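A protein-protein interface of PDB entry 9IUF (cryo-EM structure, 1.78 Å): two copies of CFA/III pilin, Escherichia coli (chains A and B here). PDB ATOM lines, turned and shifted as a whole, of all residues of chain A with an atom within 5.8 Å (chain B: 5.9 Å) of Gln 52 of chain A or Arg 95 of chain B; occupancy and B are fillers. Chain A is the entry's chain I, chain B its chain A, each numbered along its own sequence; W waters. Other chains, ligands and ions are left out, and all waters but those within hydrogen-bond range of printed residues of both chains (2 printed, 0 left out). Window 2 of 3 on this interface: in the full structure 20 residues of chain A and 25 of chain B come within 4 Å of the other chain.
The guanidinium group (NH2) of Arg 53 of chain A lies within salt-bridge range of the side-chain carboxylate (OD1) of Asp 92 of chain B (2.6 Å).
The guanidinium group (NH1) of Arg 95 of chain B is in salt-bridge range of the side-chain carboxylate (OD2) of Asp 92 of chain B (3.2 Å). The guanidinium group (NH2) of Arg 95 of chain B sits at hydrogen-bond distance from the side-chain hydroxyl (OH) of Tyr 102 of chain B, at 3.2 Å. The side-chain amide oxygen (OE1) of Gln 52 of chain A lies close to the backbone carbonyl oxygen (O) of Asp 49 of chain A (3.4 Å).
Among the printed residues, merely in contact across the chains: Gln 52 of chain A with Arg 95 of chain B (3.4 Å) and Gly 55 of chain A with Gly 100 of chain B (3.5 Å).
Gln 52 of chain A touches one residue of chain B. Printed residues of chain B within 4 Å of Arg 53 of chain A: Asp 92 (2.6 Å). Of the printed residues of chain B, Gly 55 of chain A touches Gly 100 (3.5 Å). Pro 91 of chain B touches none of the printed residues of chain A. Printed residues of chain A within 4 Å of Asp 92 of chain B: Arg 53. Of the printed residues of chain A, Arg 95 of chain B touches Gln 52 (3.4 Å). Of the printed residues of chain A, Gly 100 of chain B touches Gly 55. The nearest residue of chain B that does not touch Gln 52 of chain A is Arg 31 of chain B (4.8 Å). The nearest printed residue of chain B that does not touch Gly 55 of chain A is Asp 101 of chain B (4.9 Å).
Of the 9 printed residues of chain A, 3 touch a printed residue of chain B. Printed residues of chain A that touch a printed residue of chain B: Gln 52, Arg 53 and Gly 55. Of the 16 printed residues of chain B, 3 touch a printed residue of chain A. Printed residues of chain B that touch a printed residue of chain A: Asp 92, Arg 95 and Gly 100. Among the printed residues, 3 pairs touch across the chains. Among the printed residues, Asp or Glu carboxylates within 4 Å of a Lys or Arg side-chain nitrogen of the other chain: Arg 53 of chain A with Asp 92 of chain B.
No position is printed for both chains.
Water W1 lies within hydrogen-bond range of the backbone carbonyl oxygen (O) of Arg 53 of chain A (2.7 Å), the side-chain hydroxyl (OH) of Tyr 102 of chain B (3.1 Å) and the guanidinium group (NE) of Arg 95 of chain B (3.3 Å). Water W2 bridges the backbone NH of Ala 68 of chain B and the backbone carbonyl oxygen of Arg 53 of chain A.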
ATOM      1  N   MET A  47      -7.130   7.484 -10.511  1.00  0.00           N
ATOM      2  CA  MET A  47      -6.539   8.628 -11.193  1.00  0.00           C
ATOM      3  C   MET A  47      -6.168   9.715 -10.200  1.00  0.00           C
ATOM      4  O   MET A  47      -5.110  10.342 -10.318  1.00  0.00           O
ATOM      5  CB  MET A  47      -7.508   9.177 -12.241  1.00  0.00           C
ATOM      6  CG  MET A  47      -7.498   8.425 -13.559  1.00  0.00           C
ATOM      7  SD  MET A  47      -6.204   8.939 -14.697  1.00  0.00           S
ATOM      8  CE  MET A  47      -6.505  10.697 -14.794  1.00  0.00           C
ATOM      9  N   LYS A  48      -7.032   9.954  -9.212  1.00  0.00           N
ATOM     10  CA  LYS A  48      -6.731  10.972  -8.213  1.00  0.00           C
ATOM     11  C   LYS A  48      -5.507  10.585  -7.391  1.00  0.00           C
ATOM     12  O   LYS A  48      -4.678  11.440  -7.059  1.00  0.00           O
ATOM     13  CB  LYS A  48      -7.945  11.193  -7.316  1.00  0.00           C
ATOM     14  CG  LYS A  48      -8.849  12.312  -7.795  1.00  0.00           C
ATOM     15  CD  LYS A  48     -10.248  12.163  -7.230  1.00  0.00           C
ATOM     16  CE  LYS A  48     -10.393  12.909  -5.923  1.00  0.00           C
ATOM     17  NZ  LYS A  48     -10.195  14.368  -6.127  1.00  0.00           N
ATOM     18  N   ASP A  49      -5.373   9.300  -7.059  1.00  0.00           N
ATOM     19  CA  ASP A  49      -4.245   8.873  -6.236  1.00  0.00           C
ATOM     20  C   ASP A  49      -2.940   8.785  -7.023  1.00  0.00           C
ATOM     21  O   ASP A  49      -1.875   9.097  -6.480  1.00  0.00           O
ATOM     22  CB  ASP A  49      -4.555   7.525  -5.585  1.00  0.00           C
ATOM     23  CG  ASP A  49      -3.304   6.776  -5.177  1.00  0.00           C
ATOM     24  OD1 ASP A  49      -2.901   5.848  -5.908  1.00  0.00           O
ATOM     25  OD2 ASP A  49      -2.724   7.113  -4.126  1.00  0.00           O
ATOM     26  N   ALA A  50      -2.996   8.378  -8.293  1.00  0.00           N
ATOM     27  CA  ALA A  50      -1.785   8.048  -9.038  1.00  0.00           C
ATOM     28  C   ALA A  50      -1.016   9.276  -9.509  1.00  0.00           C
ATOM     29  O   ALA A  50       0.216   9.235  -9.577  1.00  0.00           O
ATOM     30  CB  ALA A  50      -2.134   7.170 -10.240  1.00  0.00           C
ATOM     31  N   TYR A  51      -1.708  10.365  -9.844  1.00  0.00           N
ATOM     32  CA  TYR A  51      -1.069  11.540 -10.424  1.00  0.00           C
ATOM     33  C   TYR A  51      -0.997  12.709  -9.449  1.00  0.00           C
ATOM     34  O   TYR A  51      -0.916  13.864  -9.879  1.00  0.00           O
ATOM     35  CB  TYR A  51      -1.796  11.955 -11.702  1.00  0.00           C
ATOM     36  CG  TYR A  51      -1.776  10.893 -12.776  1.00  0.00           C
ATOM     37  CD1 TYR A  51      -0.629  10.651 -13.517  1.00  0.00           C
ATOM     38  CD2 TYR A  51      -2.899  10.122 -13.038  1.00  0.00           C
ATOM     39  CE1 TYR A  51      -0.603   9.678 -14.495  1.00  0.00           C
ATOM     40  CE2 TYR A  51      -2.881   9.147 -14.012  1.00  0.00           C
ATOM     41  CZ  TYR A  51      -1.732   8.929 -14.738  1.00  0.00           C
ATOM     42  OH  TYR A  51      -1.713   7.957 -15.711  1.00  0.00           O
ATOM     43  N   GLN A  52      -1.021  12.434  -8.144  1.00  0.00           N
ATOM     44  CA  GLN A  52      -0.969  13.513  -7.163  1.00  0.00           C
ATOM     45  C   GLN A  52       0.392  14.201  -7.158  1.00  0.00           C
ATOM     46  O   GLN A  52       0.476  15.417  -6.955  1.00  0.00           O
ATOM     47  CB  GLN A  52      -1.316  12.976  -5.774  1.00  0.00           C
ATOM     48  CG  GLN A  52      -0.372  11.903  -5.260  1.00  0.00           C
ATOM     49  CD  GLN A  52      -0.895  11.221  -4.013  1.00  0.00           C
ATOM     50  OE1 GLN A  52      -0.375  10.188  -3.592  1.00  0.00           O
ATOM     51  NE2 GLN A  52      -1.930  11.796  -3.413  1.00  0.00           N
ATOM     52  N   ARG A  53       1.470  13.445  -7.378  1.00  0.00           N
ATOM     53  CA  ARG A  53       2.801  14.038  -7.384  1.00  0.00           C
ATOM     54  C   ARG A  53       3.066  14.865  -8.634  1.00  0.00           C
ATOM     55  O   ARG A  53       3.922  15.755  -8.603  1.00  0.00           O
ATOM     56  CB  ARG A  53       3.867  12.952  -7.255  1.00  0.00           C
ATOM     57  CG  ARG A  53       3.805  12.168  -5.959  1.00  0.00           C
ATOM     58  CD  ARG A  53       5.188  11.997  -5.361  1.00  0.00           C
ATOM     59  NE  ARG A  53       5.137  11.800  -3.918  1.00  0.00           N
ATOM     60  CZ  ARG A  53       5.056  10.615  -3.328  1.00  0.00           C
ATOM     61  NH1 ARG A  53       5.017   9.495  -4.031  1.00  0.00           N
ATOM     62  NH2 ARG A  53       5.012  10.553  -2.001  1.00  0.00           N
ATOM     63  N   ASP A  54       2.359  14.592  -9.730  1.00  0.00           N
ATOM     64  CA  ASP A  54       2.593  15.325 -10.967  1.00  0.00           C
ATOM     65  C   ASP A  54       1.990  16.723 -10.934  1.00  0.00           C
ATOM     66  O   ASP A  54       2.528  17.639 -11.564  1.00  0.00           O
ATOM     67  CB  ASP A  54       2.028  14.542 -12.153  1.00  0.00           C
ATOM     68  CG  ASP A  54       2.992  13.493 -12.667  1.00  0.00           C
ATOM     69  OD1 ASP A  54       4.183  13.819 -12.853  1.00  0.00           O
ATOM     70  OD2 ASP A  54       2.560  12.341 -12.882  1.00  0.00           O
ATOM     71  N   GLY A  55       0.885  16.907 -10.216  1.00  0.00           N
ATOM     72  CA  GLY A  55       0.191  18.174 -10.203  1.00  0.00           C
ATOM     73  C   GLY A  55      -0.696  18.420 -11.402  1.00  0.00           C
ATOM     74  O   GLY A  55      -1.319  19.486 -11.483  1.00  0.00           O
ATOM     75  N   ARG B  31      -9.864  14.053   4.052  1.00  0.00           N
ATOM     76  CA  ARG B  31      -8.431  13.824   4.207  1.00  0.00           C
ATOM     77  C   ARG B  31      -7.630  15.021   3.713  1.00  0.00           C
ATOM     78  O   ARG B  31      -6.695  15.477   4.384  1.00  0.00           O
ATOM     79  CB  ARG B  31      -8.012  12.555   3.464  1.00  0.00           C
ATOM     80  CG  ARG B  31      -6.592  12.112   3.775  1.00  0.00           C
ATOM     81  CD  ARG B  31      -6.146  10.966   2.882  1.00  0.00           C
ATOM     82  NE  ARG B  31      -6.354  11.257   1.470  1.00  0.00           N
ATOM     83  CZ  ARG B  31      -5.483  11.895   0.701  1.00  0.00           C
ATOM     84  NH1 ARG B  31      -4.330  12.332   1.180  1.00  0.00           N
ATOM     85  NH2 ARG B  31      -5.775  12.100  -0.579  1.00  0.00           N
ATOM     86  N   LEU B  36      -4.414  19.844   4.670  1.00  0.00           N
ATOM     87  CA  LEU B  36      -4.179  21.259   4.411  1.00  0.00           C
ATOM     88  C   LEU B  36      -4.069  22.047   5.706  1.00  0.00           C
ATOM     89  O   LEU B  36      -3.200  22.914   5.837  1.00  0.00           O
ATOM     90  CB  LEU B  36      -5.293  21.828   3.534  1.00  0.00           C
ATOM     91  CG  LEU B  36      -5.057  21.768   2.026  1.00  0.00           C
ATOM     92  CD1 LEU B  36      -6.208  22.419   1.281  1.00  0.00           C
ATOM     93  CD2 LEU B  36      -3.739  22.431   1.665  1.00  0.00           C
ATOM     94  N   ASN B  39      -0.665  21.159   7.291  1.00  0.00           N
ATOM     95  CA  ASN B  39       0.467  21.669   6.528  1.00  0.00           C
ATOM     96  C   ASN B  39       0.539  23.187   6.571  1.00  0.00           C
ATOM     97  O   ASN B  39       1.638  23.745   6.593  1.00  0.00           O
ATOM     98  CB  ASN B  39       0.390  21.174   5.086  1.00  0.00           C
ATOM     99  CG  ASN B  39       0.578  19.674   4.978  1.00  0.00           C
ATOM    100  OD1 ASN B  39       0.993  19.020   5.932  1.00  0.00           O
ATOM    101  ND2 ASN B  39       0.266  19.120   3.813  1.00  0.00           N
ATOM    102  N   ALA B  68       8.187  17.961  -8.799  1.00  0.00           N
ATOM    103  CA  ALA B  68       8.438  17.161  -7.606  1.00  0.00           C
ATOM    104  C   ALA B  68       9.912  17.162  -7.227  1.00  0.00           C
ATOM    105  O   ALA B  68      10.247  17.083  -6.039  1.00  0.00           O
ATOM    106  CB  ALA B  68       7.942  15.731  -7.820  1.00  0.00           C
ATOM    107  N   THR B  90       8.547  18.715   3.652  1.00  0.00           N
ATOM    108  CA  THR B  90       8.727  17.779   2.559  1.00  0.00           C
ATOM    109  C   THR B  90       7.918  18.228   1.352  1.00  0.00           C
ATOM    110  O   THR B  90       6.952  18.984   1.488  1.00  0.00           O
ATOM    111  CB  THR B  90       8.298  16.368   2.976  1.00  0.00           C
ATOM    112  OG1 THR B  90       6.912  16.372   3.338  1.00  0.00           O
ATOM    113  CG2 THR B  90       9.127  15.883   4.153  1.00  0.00           C
ATOM    114  N   PRO B  91       8.297  17.799   0.144  1.00  0.00           N
ATOM    115  CA  PRO B  91       7.523  18.206  -1.041  1.00  0.00           C
ATOM    116  C   PRO B  91       6.052  17.838  -0.962  1.00  0.00           C
ATOM    117  O   PRO B  91       5.203  18.601  -1.439  1.00  0.00           O
ATOM    118  CB  PRO B  91       8.235  17.473  -2.184  1.00  0.00           C
ATOM    119  CG  PRO B  91       9.634  17.320  -1.706  1.00  0.00           C
ATOM    120  CD  PRO B  91       9.541  17.099  -0.224  1.00  0.00           C
ATOM    121  N   ASP B  92       5.723  16.687  -0.373  1.00  0.00           N
ATOM    122  CA  ASP B  92       4.321  16.313  -0.219  1.00  0.00           C
ATOM    123  C   ASP B  92       3.590  17.272   0.712  1.00  0.00           C
ATOM    124  O   ASP B  92       2.440  17.641   0.450  1.00  0.00           O
ATOM    125  CB  ASP B  92       4.214  14.877   0.293  1.00  0.00           C
ATOM    126  CG  ASP B  92       4.583  13.854  -0.763  1.00  0.00           C
ATOM    127  OD1 ASP B  92       4.426  12.643  -0.501  1.00  0.00           O
ATOM    128  OD2 ASP B  92       5.028  14.260  -1.856  1.00  0.00           O
ATOM    129  N   GLU B  93       4.235  17.682   1.806  1.00  0.00           N
ATOM    130  CA  GLU B  93       3.604  18.627   2.721  1.00  0.00           C
ATOM    131  C   GLU B  93       3.501  20.018   2.114  1.00  0.00           C
ATOM    132  O   GLU B  93       2.603  20.786   2.474  1.00  0.00           O
ATOM    133  CB  GLU B  93       4.376  18.683   4.039  1.00  0.00           C
ATOM    134  CG  GLU B  93       4.312  17.405   4.854  1.00  0.00           C
ATOM    135  CD  GLU B  93       5.318  17.391   5.985  1.00  0.00           C
ATOM    136  OE1 GLU B  93       6.532  17.447   5.702  1.00  0.00           O
ATOM    137  OE2 GLU B  93       4.897  17.325   7.159  1.00  0.00           O
ATOM    138  N   ALA B  94       4.406  20.362   1.200  1.00  0.00           N
ATOM    139  CA  ALA B  94       4.386  21.666   0.552  1.00  0.00           C
ATOM    140  C   ALA B  94       3.358  21.760  -0.565  1.00  0.00           C
ATOM    141  O   ALA B  94       3.124  22.859  -1.077  1.00  0.00           O
ATOM    142  CB  ALA B  94       5.772  21.995  -0.004  1.00  0.00           C
ATOM    143  N   ARG B  95       2.740  20.649  -0.949  1.00  0.00           N
ATOM    144  CA  ARG B  95       1.830  20.606  -2.084  1.00  0.00           C
ATOM    145  C   ARG B  95       0.387  20.681  -1.606  1.00  0.00           C
ATOM    146  O   ARG B  95       0.001  19.974  -0.669  1.00  0.00           O
ATOM    147  CB  ARG B  95       2.045  19.332  -2.900  1.00  0.00           C
ATOM    148  CG  ARG B  95       1.317  19.315  -4.232  1.00  0.00           C
ATOM    149  CD  ARG B  95       1.560  18.015  -4.982  1.00  0.00           C
ATOM    150  NE  ARG B  95       2.980  17.716  -5.116  1.00  0.00           N
ATOM    151  CZ  ARG B  95       3.595  16.713  -4.506  1.00  0.00           C
ATOM    152  NH1 ARG B  95       2.942  15.885  -3.708  1.00  0.00           N
ATOM    153  NH2 ARG B  95       4.898  16.537  -4.699  1.00  0.00           N
ATOM    154  N   ASN B  96      -0.400  21.538  -2.249  1.00  0.00           N
ATOM    155  CA  ASN B  96      -1.839  21.577  -2.017  1.00  0.00           C
ATOM    156  C   ASN B  96      -2.450  20.303  -2.585  1.00  0.00           C
ATOM    157  O   ASN B  96      -2.413  20.075  -3.798  1.00  0.00           O
ATOM    158  CB  ASN B  96      -2.438  22.823  -2.668  1.00  0.00           C
ATOM    159  CG  ASN B  96      -3.911  23.016  -2.344  1.00  0.00           C
ATOM    160  OD1 ASN B  96      -4.642  22.062  -2.083  1.00  0.00           O
ATOM    161  ND2 ASN B  96      -4.353  24.266  -2.365  1.00  0.00           N
ATOM    162  N   GLY B  97      -3.016  19.471  -1.713  1.00  0.00           N
ATOM    163  CA  GLY B  97      -3.549  18.193  -2.148  1.00  0.00           C
ATOM    164  C   GLY B  97      -4.816  18.283  -2.970  1.00  0.00           C
ATOM    165  O   GLY B  97      -5.217  17.278  -3.566  1.00  0.00           O
ATOM    166  N   GLY B 100      -3.216  20.472  -6.479  1.00  0.00           N
ATOM    167  CA  GLY B 100      -2.007  19.888  -7.016  1.00  0.00           C
ATOM    168  C   GLY B 100      -0.844  20.843  -7.151  1.00  0.00           C
ATOM    169  O   GLY B 100       0.237  20.416  -7.577  1.00  0.00           O
ATOM    170  N   ASP B 101      -1.023  22.112  -6.805  1.00  0.00           N
ATOM    171  CA  ASP B 101       0.047  23.092  -6.872  1.00  0.00           C
ATOM    172  C   ASP B 101       0.756  23.192  -5.532  1.00  0.00           C
ATOM    173  O   ASP B 101       0.181  22.906  -4.479  1.00  0.00           O
ATOM    174  CB  ASP B 101      -0.496  24.466  -7.266  1.00  0.00           C
ATOM    175  CG  ASP B 101      -1.194  24.458  -8.607  1.00  0.00           C
ATOM    176  OD1 ASP B 101      -0.604  23.951  -9.583  1.00  0.00           O
ATOM    177  OD2 ASP B 101      -2.335  24.956  -8.682  1.00  0.00           O
ATOM    178  N   TYR B 102       2.021  23.592  -5.579  1.00  0.00           N
ATOM    179  CA  TYR B 102       2.732  23.911  -4.352  1.00  0.00           C
ATOM    180  C   TYR B 102       2.165  25.189  -3.752  1.00  0.00           C
ATOM    181  O   TYR B 102       1.766  26.108  -4.473  1.00  0.00           O
ATOM    182  CB  TYR B 102       4.226  24.048  -4.623  1.00  0.00           C
ATOM    183  CG  TYR B 102       4.881  22.723  -4.919  1.00  0.00           C
ATOM    184  CD1 TYR B 102       5.043  21.772  -3.922  1.00  0.00           C
ATOM    185  CD2 TYR B 102       5.321  22.413  -6.197  1.00  0.00           C
ATOM    186  CE1 TYR B 102       5.632  20.555  -4.186  1.00  0.00           C
ATOM    187  CE2 TYR B 102       5.913  21.197  -6.471  1.00  0.00           C
ATOM    188  CZ  TYR B 102       6.065  20.272  -5.461  1.00  0.00           C
ATOM    189  OH  TYR B 102       6.652  19.059  -5.723  1.00  0.00           O
ATOM    190  N   ILE B 103       2.120  25.240  -2.423  1.00  0.00           N
ATOM    191  CA  ILE B 103       1.425  26.322  -1.737  1.00  0.00           C
ATOM    192  C   ILE B 103       2.143  27.637  -1.996  1.00  0.00           C
ATOM    193  O   ILE B 103       3.361  27.750  -1.807  1.00  0.00           O
ATOM    194  CB  ILE B 103       1.318  26.021  -0.235  1.00  0.00           C
ATOM    195  CG1 ILE B 103       0.261  24.941   0.005  1.00  0.00           C
ATOM    196  CG2 ILE B 103       0.981  27.280   0.542  1.00  0.00           C
ATOM    197  CD1 ILE B 103       0.381  24.250   1.339  1.00  0.00           C
HETATM  198  O   HOH W   1       4.671  18.224  -7.935  1.00  0.00           O
HETATM  199  O   HOH W   2       6.343  16.762 -10.602  1.00  0.00           O
